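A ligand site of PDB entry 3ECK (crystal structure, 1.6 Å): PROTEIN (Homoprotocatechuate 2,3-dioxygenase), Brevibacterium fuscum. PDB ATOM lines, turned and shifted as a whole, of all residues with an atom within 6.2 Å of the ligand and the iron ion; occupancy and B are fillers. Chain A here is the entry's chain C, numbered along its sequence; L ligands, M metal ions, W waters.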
ATOM      1  N   HIS A 155      16.147   2.067  -2.734  1.00  0.00           N
ATOM      2  CA  HIS A 155      17.445   1.926  -3.399  1.00  0.00           C
ATOM      3  C   HIS A 155      18.591   1.525  -2.479  1.00  0.00           C
ATOM      4  O   HIS A 155      18.470   1.585  -1.256  1.00  0.00           O
ATOM      5  CB  HIS A 155      17.816   3.216  -4.162  1.00  0.00           C
ATOM      6  CG  HIS A 155      18.084   4.418  -3.277  1.00  0.00           C
ATOM      7  ND1 HIS A 155      17.123   5.369  -3.004  1.00  0.00           N
ATOM      8  CD2 HIS A 155      19.221   4.843  -2.684  1.00  0.00           C
ATOM      9  CE1 HIS A 155      17.660   6.327  -2.250  1.00  0.00           C
ATOM     10  NE2 HIS A 155      18.929   6.027  -2.045  1.00  0.00           N
ATOM     11  N   PHE A 156      19.695   1.125  -3.098  1.00  0.00           N
ATOM     12  CA  PHE A 156      20.965   0.947  -2.405  1.00  0.00           C
ATOM     13  C   PHE A 156      21.929   2.047  -2.862  1.00  0.00           C
ATOM     14  O   PHE A 156      21.723   2.680  -3.899  1.00  0.00           O
ATOM     15  CB  PHE A 156      21.592  -0.395  -2.780  1.00  0.00           C
ATOM     16  CG  PHE A 156      20.666  -1.573  -2.645  1.00  0.00           C
ATOM     17  CD1 PHE A 156      20.018  -1.849  -1.436  1.00  0.00           C
ATOM     18  CD2 PHE A 156      20.473  -2.434  -3.722  1.00  0.00           C
ATOM     19  CE1 PHE A 156      19.197  -2.975  -1.309  1.00  0.00           C
ATOM     20  CE2 PHE A 156      19.660  -3.551  -3.608  1.00  0.00           C
ATOM     21  CZ  PHE A 156      19.008  -3.821  -2.406  1.00  0.00           C
ATOM     22  N   ASN A 157      22.984   2.275  -2.093  1.00  0.00           N
ATOM     23  CA  ASN A 157      24.029   3.198  -2.540  1.00  0.00           C
ATOM     24  C   ASN A 157      25.384   2.594  -2.155  1.00  0.00           C
ATOM     25  O   ASN A 157      25.613   2.278  -0.982  1.00  0.00           O
ATOM     26  CB  ASN A 157      23.844   4.604  -1.964  1.00  0.00           C
ATOM     27  CG  ASN A 157      24.848   5.595  -2.534  1.00  0.00           C
ATOM     28  OD1 ASN A 157      26.071   5.358  -2.466  1.00  0.00           O
ATOM     29  ND2 ASN A 157      24.357   6.705  -3.111  1.00  0.00           N
ATOM     30  N   ILE A 181      27.415  13.437 -10.734  1.00  0.00           N
ATOM     31  CA  ILE A 181      28.197  14.592 -10.280  1.00  0.00           C
ATOM     32  C   ILE A 181      29.585  14.494 -10.905  1.00  0.00           C
ATOM     33  O   ILE A 181      30.242  13.449 -10.788  1.00  0.00           O
ATOM     34  CB  ILE A 181      28.287  14.616  -8.749  1.00  0.00           C
ATOM     35  CG1 ILE A 181      26.884  14.781  -8.158  1.00  0.00           C
ATOM     36  CG2 ILE A 181      29.178  15.757  -8.290  1.00  0.00           C
ATOM     37  CD1 ILE A 181      26.846  14.751  -6.635  1.00  0.00           C
ATOM     38  N   TRP A 192      23.896   7.880 -10.424  1.00  0.00           N
ATOM     39  CA  TRP A 192      22.643   7.248  -9.966  1.00  0.00           C
ATOM     40  C   TRP A 192      22.047   6.500 -11.154  1.00  0.00           C
ATOM     41  O   TRP A 192      22.056   7.011 -12.279  1.00  0.00           O
ATOM     42  CB  TRP A 192      21.647   8.322  -9.529  1.00  0.00           C
ATOM     43  CG  TRP A 192      21.940   8.934  -8.185  1.00  0.00           C
ATOM     44  CD1 TRP A 192      21.244   8.705  -7.023  1.00  0.00           C
ATOM     45  CD2 TRP A 192      22.979   9.883  -7.850  1.00  0.00           C
ATOM     46  NE1 TRP A 192      21.780   9.446  -5.997  1.00  0.00           N
ATOM     47  CE2 TRP A 192      22.846  10.175  -6.469  1.00  0.00           C
ATOM     48  CE3 TRP A 192      24.003  10.502  -8.575  1.00  0.00           C
ATOM     49  CZ2 TRP A 192      23.701  11.061  -5.796  1.00  0.00           C
ATOM     50  CZ3 TRP A 192      24.858  11.418  -7.905  1.00  0.00           C
ATOM     51  CH2 TRP A 192      24.706  11.672  -6.530  1.00  0.00           C
ATOM     52  N   VAL A 199      14.383   7.522  -9.654  1.00  0.00           N
ATOM     53  CA  VAL A 199      15.704   8.089  -9.930  1.00  0.00           C
ATOM     54  C   VAL A 199      16.784   7.029  -9.853  1.00  0.00           C
ATOM     55  O   VAL A 199      17.752   7.070 -10.629  1.00  0.00           O
ATOM     56  CB  VAL A 199      16.032   9.296  -9.020  1.00  0.00           C
ATOM     57  CG1 VAL A 199      17.493   9.733  -9.176  1.00  0.00           C
ATOM     58  CG2 VAL A 199      15.125  10.434  -9.384  1.00  0.00           C
ATOM     59  N   HIS A 200      16.621   6.064  -8.948  1.00  0.00           N
ATOM     60  CA  HIS A 200      17.568   4.957  -8.885  1.00  0.00           C
ATOM     61  C   HIS A 200      17.122   3.723  -8.155  1.00  0.00           C
ATOM     62  O   HIS A 200      16.206   3.778  -7.327  1.00  0.00           O
ATOM     63  CB  HIS A 200      18.957   5.393  -8.360  1.00  0.00           C
ATOM     64  CG  HIS A 200      18.963   6.025  -6.989  1.00  0.00           C
ATOM     65  ND1 HIS A 200      18.020   6.944  -6.576  1.00  0.00           N
ATOM     66  CD2 HIS A 200      19.875   5.932  -5.993  1.00  0.00           C
ATOM     67  CE1 HIS A 200      18.337   7.365  -5.364  1.00  0.00           C
ATOM     68  NE2 HIS A 200      19.460   6.776  -4.992  1.00  0.00           N
ATOM     69  N   ALA A 203      23.226   3.185  -6.738  1.00  0.00           N
ATOM     70  CA  ALA A 203      24.035   4.362  -7.052  1.00  0.00           C
ATOM     71  C   ALA A 203      25.468   4.058  -6.673  1.00  0.00           C
ATOM     72  O   ALA A 203      25.739   3.218  -5.824  1.00  0.00           O
ATOM     73  CB  ALA A 203      23.546   5.583  -6.292  1.00  0.00           C
ATOM     74  N   THR A 205      28.856   5.978  -5.259  1.00  0.00           N
ATOM     75  CA  THR A 205      29.495   7.128  -4.608  1.00  0.00           C
ATOM     76  C   THR A 205      31.009   6.883  -4.651  1.00  0.00           C
ATOM     77  O   THR A 205      31.459   5.833  -4.219  1.00  0.00           O
ATOM     78  CB  THR A 205      29.051   7.243  -3.120  1.00  0.00           C
ATOM     79  OG1 THR A 205      27.620   7.438  -3.056  1.00  0.00           O
ATOM     80  CG2 THR A 205      29.737   8.407  -2.428  1.00  0.00           C
ATOM     81  N   HIS A 213      27.187   2.241   1.221  1.00  0.00           N
ATOM     82  CA  HIS A 213      26.925   3.556   1.780  1.00  0.00           C
ATOM     83  C   HIS A 213      25.627   3.579   2.594  1.00  0.00           C
ATOM     84  O   HIS A 213      25.650   3.937   3.765  1.00  0.00           O
ATOM     85  CB  HIS A 213      26.910   4.665   0.733  1.00  0.00           C
ATOM     86  CG  HIS A 213      27.095   6.011   1.338  1.00  0.00           C
ATOM     87  ND1 HIS A 213      26.061   6.694   1.942  1.00  0.00           N
ATOM     88  CD2 HIS A 213      28.199   6.780   1.496  1.00  0.00           C
ATOM     89  CE1 HIS A 213      26.515   7.837   2.423  1.00  0.00           C
ATOM     90  NE2 HIS A 213      27.808   7.916   2.159  1.00  0.00           N
ATOM     91  N   HIS A 214      24.536   3.169   1.970  1.00  0.00           N
ATOM     92  CA  HIS A 214      23.235   3.100   2.671  1.00  0.00           C
ATOM     93  C   HIS A 214      22.201   2.253   1.943  1.00  0.00           C
ATOM     94  O   HIS A 214      22.398   1.910   0.773  1.00  0.00           O
ATOM     95  CB  HIS A 214      22.662   4.512   2.923  1.00  0.00           C
ATOM     96  CG  HIS A 214      22.437   5.338   1.682  1.00  0.00           C
ATOM     97  ND1 HIS A 214      23.367   6.240   1.218  1.00  0.00           N
ATOM     98  CD2 HIS A 214      21.357   5.443   0.855  1.00  0.00           C
ATOM     99  CE1 HIS A 214      22.887   6.847   0.146  1.00  0.00           C
ATOM    100  NE2 HIS A 214      21.671   6.389  -0.092  1.00  0.00           N
ATOM    101  N   ALA A 216      18.001   2.682   1.340  1.00  0.00           N
ATOM    102  CA  ALA A 216      16.980   3.747   1.438  1.00  0.00           C
ATOM    103  C   ALA A 216      15.580   3.174   1.430  1.00  0.00           C
ATOM    104  O   ALA A 216      15.252   2.325   0.574  1.00  0.00           O
ATOM    105  CB  ALA A 216      17.114   4.729   0.312  1.00  0.00           C
ATOM    106  N   ARG A 243      22.655  13.167   9.077  1.00  0.00           N
ATOM    107  CA  ARG A 243      22.607  14.211   8.083  1.00  0.00           C
ATOM    108  C   ARG A 243      21.163  14.428   7.677  1.00  0.00           C
ATOM    109  O   ARG A 243      20.452  13.454   7.417  1.00  0.00           O
ATOM    110  CB  ARG A 243      23.421  13.816   6.846  1.00  0.00           C
ATOM    111  CG  ARG A 243      23.282  14.821   5.727  1.00  0.00           C
ATOM    112  CD  ARG A 243      24.075  14.464   4.479  1.00  0.00           C
ATOM    113  NE  ARG A 243      23.543  15.250   3.378  1.00  0.00           N
ATOM    114  CZ  ARG A 243      23.584  14.922   2.086  1.00  0.00           C
ATOM    115  NH1 ARG A 243      24.190  13.819   1.656  1.00  0.00           N
ATOM    116  NH2 ARG A 243      22.981  15.722   1.211  1.00  0.00           N
ATOM    117  N   ARG A 247      16.360  18.601   1.366  1.00  0.00           N
ATOM    118  CA  ARG A 247      15.936  18.382   0.002  1.00  0.00           C
ATOM    119  C   ARG A 247      17.200  18.109  -0.776  1.00  0.00           C
ATOM    120  O   ARG A 247      18.141  18.897  -0.733  1.00  0.00           O
ATOM    121  CB  ARG A 247      15.258  19.654  -0.544  1.00  0.00           C
ATOM    122  CG  ARG A 247      14.983  19.628  -2.044  1.00  0.00           C
ATOM    123  CD  ARG A 247      13.831  18.707  -2.369  1.00  0.00           C
ATOM    124  NE  ARG A 247      12.569  19.259  -1.882  1.00  0.00           N
ATOM    125  CZ  ARG A 247      11.388  18.638  -2.004  1.00  0.00           C
ATOM    126  NH1 ARG A 247      11.315  17.423  -2.535  1.00  0.00           N
ATOM    127  NH2 ARG A 247      10.298  19.228  -1.523  1.00  0.00           N
ATOM    128  N   HIS A 248      17.234  16.978  -1.482  1.00  0.00           N
ATOM    129  CA  HIS A 248      18.356  16.684  -2.365  1.00  0.00           C
ATOM    130  C   HIS A 248      18.310  17.571  -3.608  1.00  0.00           C
ATOM    131  O   HIS A 248      17.241  17.909  -4.109  1.00  0.00           O
ATOM    132  CB  HIS A 248      18.309  15.223  -2.834  1.00  0.00           C
ATOM    133  CG  HIS A 248      18.776  14.216  -1.830  1.00  0.00           C
ATOM    134  ND1 HIS A 248      19.977  14.336  -1.152  1.00  0.00           N
ATOM    135  CD2 HIS A 248      18.246  13.036  -1.435  1.00  0.00           C
ATOM    136  CE1 HIS A 248      20.155  13.284  -0.373  1.00  0.00           C
ATOM    137  NE2 HIS A 248      19.129  12.463  -0.540  1.00  0.00           N
ATOM    138  N   GLY A 249      19.478  17.922  -4.130  1.00  0.00           N
ATOM    139  CA  GLY A 249      19.546  18.485  -5.459  1.00  0.00           C
ATOM    140  C   GLY A 249      19.403  17.332  -6.443  1.00  0.00           C
ATOM    141  O   GLY A 249      18.349  17.186  -7.109  1.00  0.00           O
ATOM    142  N   VAL A 250      20.431  16.487  -6.497  1.00  0.00           N
ATOM    143  CA  VAL A 250      20.324  15.237  -7.264  1.00  0.00           C
ATOM    144  C   VAL A 250      19.080  14.480  -6.743  1.00  0.00           C
ATOM    145  O   VAL A 250      18.933  14.321  -5.537  1.00  0.00           O
ATOM    146  CB  VAL A 250      21.575  14.341  -7.075  1.00  0.00           C
ATOM    147  CG1 VAL A 250      21.328  12.954  -7.661  1.00  0.00           C
ATOM    148  CG2 VAL A 250      22.804  15.003  -7.702  1.00  0.00           C
ATOM    149  N   SER A 251      18.219  14.048  -7.663  1.00  0.00           N
ATOM    150  CA  SER A 251      16.995  13.267  -7.344  1.00  0.00           C
ATOM    151  C   SER A 251      15.785  14.097  -6.910  1.00  0.00           C
ATOM    152  O   SER A 251      14.669  13.627  -7.029  1.00  0.00           O
ATOM    153  CB  SER A 251      17.246  12.158  -6.303  1.00  0.00           C
ATOM    154  OG  SER A 251      17.114  12.652  -4.981  1.00  0.00           O
ATOM    155  N   ASN A 252      16.021  15.303  -6.392  1.00  0.00           N
ATOM    156  CA  ASN A 252      14.956  16.189  -5.899  1.00  0.00           C
ATOM    157  C   ASN A 252      14.165  15.611  -4.703  1.00  0.00           C
ATOM    158  O   ASN A 252      13.119  16.162  -4.332  1.00  0.00           O
ATOM    159  CB  ASN A 252      13.974  16.548  -7.043  1.00  0.00           C
ATOM    160  CG  ASN A 252      13.034  17.710  -6.683  1.00  0.00           C
ATOM    161  OD1 ASN A 252      13.431  18.681  -6.064  1.00  0.00           O
ATOM    162  ND2 ASN A 252      11.762  17.582  -7.095  1.00  0.00           N
ATOM    163  N   ALA A 253      14.634  14.509  -4.120  1.00  0.00           N
ATOM    164  CA  ALA A 253      13.912  13.876  -3.006  1.00  0.00           C
ATOM    165  C   ALA A 253      14.150  14.574  -1.655  1.00  0.00           C
ATOM    166  O   ALA A 253      15.211  15.139  -1.426  1.00  0.00           O
ATOM    167  CB  ALA A 253      14.260  12.409  -2.900  1.00  0.00           C
ATOM    168  N   TYR A 255      14.854  14.035   2.228  1.00  0.00           N
ATOM    169  CA  TYR A 255      15.662  12.938   2.755  1.00  0.00           C
ATOM    170  C   TYR A 255      16.092  13.116   4.214  1.00  0.00           C
ATOM    171  O   TYR A 255      16.012  14.222   4.778  1.00  0.00           O
ATOM    172  CB  TYR A 255      16.930  12.759   1.926  1.00  0.00           C
ATOM    173  CG  TYR A 255      17.932  13.886   2.161  1.00  0.00           C
ATOM    174  CD1 TYR A 255      17.916  15.034   1.362  1.00  0.00           C
ATOM    175  CD2 TYR A 255      18.885  13.802   3.182  1.00  0.00           C
ATOM    176  CE1 TYR A 255      18.847  16.095   1.569  1.00  0.00           C
ATOM    177  CE2 TYR A 255      19.814  14.849   3.395  1.00  0.00           C
ATOM    178  CZ  TYR A 255      19.784  15.987   2.579  1.00  0.00           C
ATOM    179  OH  TYR A 255      20.696  16.987   2.820  1.00  0.00           O
ATOM    180  N   TYR A 257      19.287  10.920   6.763  1.00  0.00           N
ATOM    181  CA  TYR A 257      20.134   9.733   7.016  1.00  0.00           C
ATOM    182  C   TYR A 257      20.315   9.496   8.490  1.00  0.00           C
ATOM    183  O   TYR A 257      20.658  10.425   9.243  1.00  0.00           O
ATOM    184  CB  TYR A 257      21.534   9.872   6.402  1.00  0.00           C
ATOM    185  CG  TYR A 257      21.512  10.134   4.920  1.00  0.00           C
ATOM    186  CD1 TYR A 257      21.595   9.064   4.011  1.00  0.00           C
ATOM    187  CD2 TYR A 257      21.422  11.435   4.415  1.00  0.00           C
ATOM    188  CE1 TYR A 257      21.580   9.297   2.633  1.00  0.00           C
ATOM    189  CE2 TYR A 257      21.396  11.676   3.052  1.00  0.00           C
ATOM    190  CZ  TYR A 257      21.488  10.595   2.156  1.00  0.00           C
ATOM    191  OH  TYR A 257      21.479  10.859   0.819  1.00  0.00           O
ATOM    192  N   GLU A 267      18.806   5.603   4.760  1.00  0.00           N
ATOM    193  CA  GLU A 267      18.207   6.837   4.278  1.00  0.00           C
ATOM    194  C   GLU A 267      16.691   6.683   4.262  1.00  0.00           C
ATOM    195  O   GLU A 267      16.187   5.611   3.908  1.00  0.00           O
ATOM    196  CB  GLU A 267      18.682   7.187   2.876  1.00  0.00           C
ATOM    197  CG  GLU A 267      18.220   8.573   2.380  1.00  0.00           C
ATOM    198  CD  GLU A 267      18.665   8.857   0.953  1.00  0.00           C
ATOM    199  OE1 GLU A 267      19.199   7.936   0.299  1.00  0.00           O
ATOM    200  OE2 GLU A 267      18.488   9.995   0.478  1.00  0.00           O
ATOM    201  N   TYR A 269      13.472   8.620   2.399  1.00  0.00           N
ATOM    202  CA  TYR A 269      13.521   9.270   1.102  1.00  0.00           C
ATOM    203  C   TYR A 269      12.080   9.427   0.610  1.00  0.00           C
ATOM    204  O   TYR A 269      11.263   8.542   0.833  1.00  0.00           O
ATOM    205  CB  TYR A 269      14.304   8.310   0.202  1.00  0.00           C
ATOM    206  CG  TYR A 269      14.595   8.672  -1.232  1.00  0.00           C
ATOM    207  CD1 TYR A 269      15.807   9.297  -1.594  1.00  0.00           C
ATOM    208  CD2 TYR A 269      13.709   8.331  -2.263  1.00  0.00           C
ATOM    209  CE1 TYR A 269      16.123   9.570  -2.945  1.00  0.00           C
ATOM    210  CE2 TYR A 269      14.011   8.589  -3.603  1.00  0.00           C
ATOM    211  CZ  TYR A 269      15.222   9.213  -3.951  1.00  0.00           C
ATOM    212  OH  TYR A 269      15.529   9.474  -5.262  1.00  0.00           O
ATOM    213  N   ARG A 292      23.886  20.855  -4.875  1.00  0.00           N
ATOM    214  CA  ARG A 292      23.772  19.573  -5.589  1.00  0.00           C
ATOM    215  C   ARG A 292      23.337  18.433  -4.646  1.00  0.00           C
ATOM    216  O   ARG A 292      22.618  17.513  -5.064  1.00  0.00           O
ATOM    217  CB  ARG A 292      25.081  19.182  -6.308  1.00  0.00           C
ATOM    218  CG  ARG A 292      26.136  18.660  -5.331  1.00  0.00           C
ATOM    219  CD  ARG A 292      27.607  18.642  -5.834  1.00  0.00           C
ATOM    220  NE  ARG A 292      28.434  18.120  -4.750  1.00  0.00           N
ATOM    221  CZ  ARG A 292      28.819  18.821  -3.674  1.00  0.00           C
ATOM    222  NH1 ARG A 292      28.504  20.117  -3.550  1.00  0.00           N
ATOM    223  NH2 ARG A 292      29.530  18.226  -2.715  1.00  0.00           N
ATOM    224  N   ARG A 293      23.807  18.478  -3.395  1.00  0.00           N
ATOM    225  CA  ARG A 293      23.548  17.398  -2.440  1.00  0.00           C
ATOM    226  C   ARG A 293      22.434  17.782  -1.466  1.00  0.00           C
ATOM    227  O   ARG A 293      21.498  17.009  -1.243  1.00  0.00           O
ATOM    228  CB  ARG A 293      24.816  16.952  -1.718  1.00  0.00           C
ATOM    229  CG  ARG A 293      25.698  16.099  -2.648  1.00  0.00           C
ATOM    230  CD  ARG A 293      26.608  15.191  -1.910  1.00  0.00           C
ATOM    231  NE  ARG A 293      27.445  14.360  -2.790  1.00  0.00           N
ATOM    232  CZ  ARG A 293      27.152  13.123  -3.223  1.00  0.00           C
ATOM    233  NH1 ARG A 293      25.978  12.558  -2.922  1.00  0.00           N
ATOM    234  NH2 ARG A 293      28.021  12.472  -3.990  1.00  0.00           N
ATOM    235  N   ASP A 294      22.559  18.976  -0.885  1.00  0.00           N
ATOM    236  CA  ASP A 294      21.446  19.574  -0.169  1.00  0.00           C
ATOM    237  C   ASP A 294      21.082  20.847  -0.923  1.00  0.00           C
ATOM    238  O   ASP A 294      21.898  21.773  -1.048  1.00  0.00           O
ATOM    239  CB  ASP A 294      21.806  19.872   1.281  1.00  0.00           C
ATOM    240  CG  ASP A 294      20.611  20.339   2.053  1.00  0.00           C
ATOM    241  OD1 ASP A 294      19.845  19.465   2.538  1.00  0.00           O
ATOM    242  OD2 ASP A 294      20.414  21.574   2.148  1.00  0.00           O
ATOM    243  N   VAL A 300      27.347  19.172   3.984  1.00  0.00           N
ATOM    244  CA  VAL A 300      27.371  17.721   4.050  1.00  0.00           C
ATOM    245  C   VAL A 300      28.376  17.291   5.128  1.00  0.00           C
ATOM    246  O   VAL A 300      29.581  17.541   4.988  1.00  0.00           O
ATOM    247  CB  VAL A 300      27.701  17.068   2.690  1.00  0.00           C
ATOM    248  CG1 VAL A 300      27.741  15.538   2.839  1.00  0.00           C
ATOM    249  CG2 VAL A 300      26.682  17.484   1.609  1.00  0.00           C
ATOM    250  N   TRP A 304      29.571  11.504   6.286  1.00  0.00           N
ATOM    251  CA  TRP A 304      28.785  11.051   5.147  1.00  0.00           C
ATOM    252  C   TRP A 304      29.687  10.666   3.980  1.00  0.00           C
ATOM    253  O   TRP A 304      29.383   9.724   3.235  1.00  0.00           O
ATOM    254  CB  TRP A 304      27.770  12.111   4.723  1.00  0.00           C
ATOM    255  CG  TRP A 304      26.629  11.539   3.924  1.00  0.00           C
ATOM    256  CD1 TRP A 304      25.443  11.065   4.421  1.00  0.00           C
ATOM    257  CD2 TRP A 304      26.587  11.366   2.511  1.00  0.00           C
ATOM    258  NE1 TRP A 304      24.643  10.622   3.375  1.00  0.00           N
ATOM    259  CE2 TRP A 304      25.324  10.799   2.191  1.00  0.00           C
ATOM    260  CE3 TRP A 304      27.485  11.653   1.463  1.00  0.00           C
ATOM    261  CZ2 TRP A 304      24.944  10.491   0.897  1.00  0.00           C
ATOM    262  CZ3 TRP A 304      27.094  11.346   0.147  1.00  0.00           C
ATOM    263  CH2 TRP A 304      25.837  10.761  -0.118  1.00  0.00           C
HETATM  264  O1  LIG L   1      19.326   9.103  -2.525  1.00  0.00           O
HETATM  265  C1  LIG L   1      20.198   9.965  -2.927  1.00  0.00           C
HETATM  266  C2  LIG L   1      21.598  10.004  -2.304  1.00  0.00           C
HETATM  267  O2  LIG L   1      22.726   9.610  -3.085  1.00  0.00           O
HETATM  268  O3  LIG L   1      21.719   9.249  -1.096  1.00  0.00           O
HETATM  269  C3  LIG L   1      22.075  11.378  -2.141  1.00  0.00           C
HETATM  270  C4  LIG L   1      19.821  10.973  -3.825  1.00  0.00           C
HETATM  271  C5  LIG L   1      20.548  12.169  -3.869  1.00  0.00           C
HETATM  272  C6  LIG L   1      21.670  12.360  -3.058  1.00  0.00           C
HETATM  273  S1  LIG L   1      22.489  13.737  -3.030  1.00  0.00           S
HETATM  274  O4  LIG L   1      21.638  14.845  -3.458  1.00  0.00           O
HETATM  275  O5  LIG L   1      23.608  13.620  -3.961  1.00  0.00           O
HETATM  276  O6  LIG L   1      23.081  14.003  -1.463  1.00  0.00           O
HETATM  277 FE    FE M   1      20.306   7.575  -1.344  1.00  0.00          FE
HETATM  278  O   HOH W   1      21.590   7.180  -3.166  1.00  0.00           O
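An oxygen (O4) of the ligand lies close to the backbone carbonyl oxygen (O) of Val 250 (3.5 Å). O4 of the ligand lies close to O of Arg 292, 3.3 Å away. Gly 249 touches the ligand (N to O4, 3.8 Å). Ser 251 touches the ligand (OG to C4, 3.4 Å). CE1 of Tyr 269 touches O1 of the ligand (3.3 Å). Trp 304 touches the ligand (CZ2 to O3, 3.99 Å). Hydrophobic or aromatic side chains within 4 Å of the ligand: His 155, Trp 192, His 200, His 214, His 248, Val 250, Tyr 257, Tyr 269 and Trp 304. 16 residues have an atom within 4 Å of the ligand: His 155, Asn 157, Trp 192, His 200, His 214, Arg 243, His 248, Gly 249, Val 250, Ser 251, Tyr 257, Glu 267, Tyr 269, Arg 292, Arg 293 and Trp 304. The nearest printed residue that does not touch the ligand is Ile 181 (4.3 Å).
Water W1 lies within hydrogen-bond range of O2 of the ligand, ND2 of Asn 157 and NE2 of His 200.
An oxygen (O5) of the ligand is in salt-bridge range of the guanidinium group (NH1) of Arg 293, at 2.8 Å. An oxygen (O1) of the ligand sits close to a ring nitrogen (NE2) of His 200 (3.4 Å). An oxygen (O2) of the ligand sits at hydrogen-bond distance from the indole nitrogen (NE1) of Trp 192. An oxygen (O2) of the ligand is in hydrogen-bond range of the side-chain amide nitrogen (ND2) of Asn 157 (3.3 Å). An oxygen (O4) of the ligand is in hydrogen-bond range of a ring nitrogen (ND1) of His 248 (2.9 Å). The side-chain hydroxyl of Tyr 257 lies close to an oxygen (O3) of the ligand, at 2.5 Å. NH2 of Arg 243 is in hydrogen-bond range of O6 of the ligand, 3.2 Å away.
His 200 touches the iron ion (NE2 to FE, 3.8 Å). Four residues have an atom within 4 Å of the iron ion: His 155, His 200, His 214 and Glu 267. The nearest printed residue that does not touch the iron ion is Tyr 257 (4.1 Å).
The backbone carbonyl oxygen (O) of Arg 292 lies close to the backbone NH (N) of Gly 249, at 3.3 Å. The backbone NH (N) of His 248 lies within hydrogen-bond range of the backbone carbonyl oxygen (O) of Ala 253 (2.7 Å). The backbone carbonyl oxygen of Arg 293 lies within hydrogen-bond range of a ring nitrogen (ND1) of His 248 (3.1 Å). The guanidinium group (NH2) of Arg 243 lies within hydrogen-bond range of the side-chain hydroxyl (OH) of Tyr 255, 3.1 Å away. The side-chain amide oxygen (OD1) of Asn 157 lies within hydrogen-bond range of the side-chain hydroxyl (OG1) of Thr 205, 2.7 Å away. OE2 of Glu 267 sits at hydrogen-bond distance from OH of Tyr 257, 3.1 Å away. The backbone carbonyl oxygen of Arg 243 sits at hydrogen-bond distance from the backbone NH of Tyr 257 (2.9 Å). O of Arg 293 lies within hydrogen-bond range of NH2 of Arg 243, at 3.1 Å.
The iron ion is bound by OE1 of Glu 267, O1 of the ligand, NE2 of His 155, NE2 of His 214, O3 of the ligand and water W1. The iron ion has six donor atoms within binding distance.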
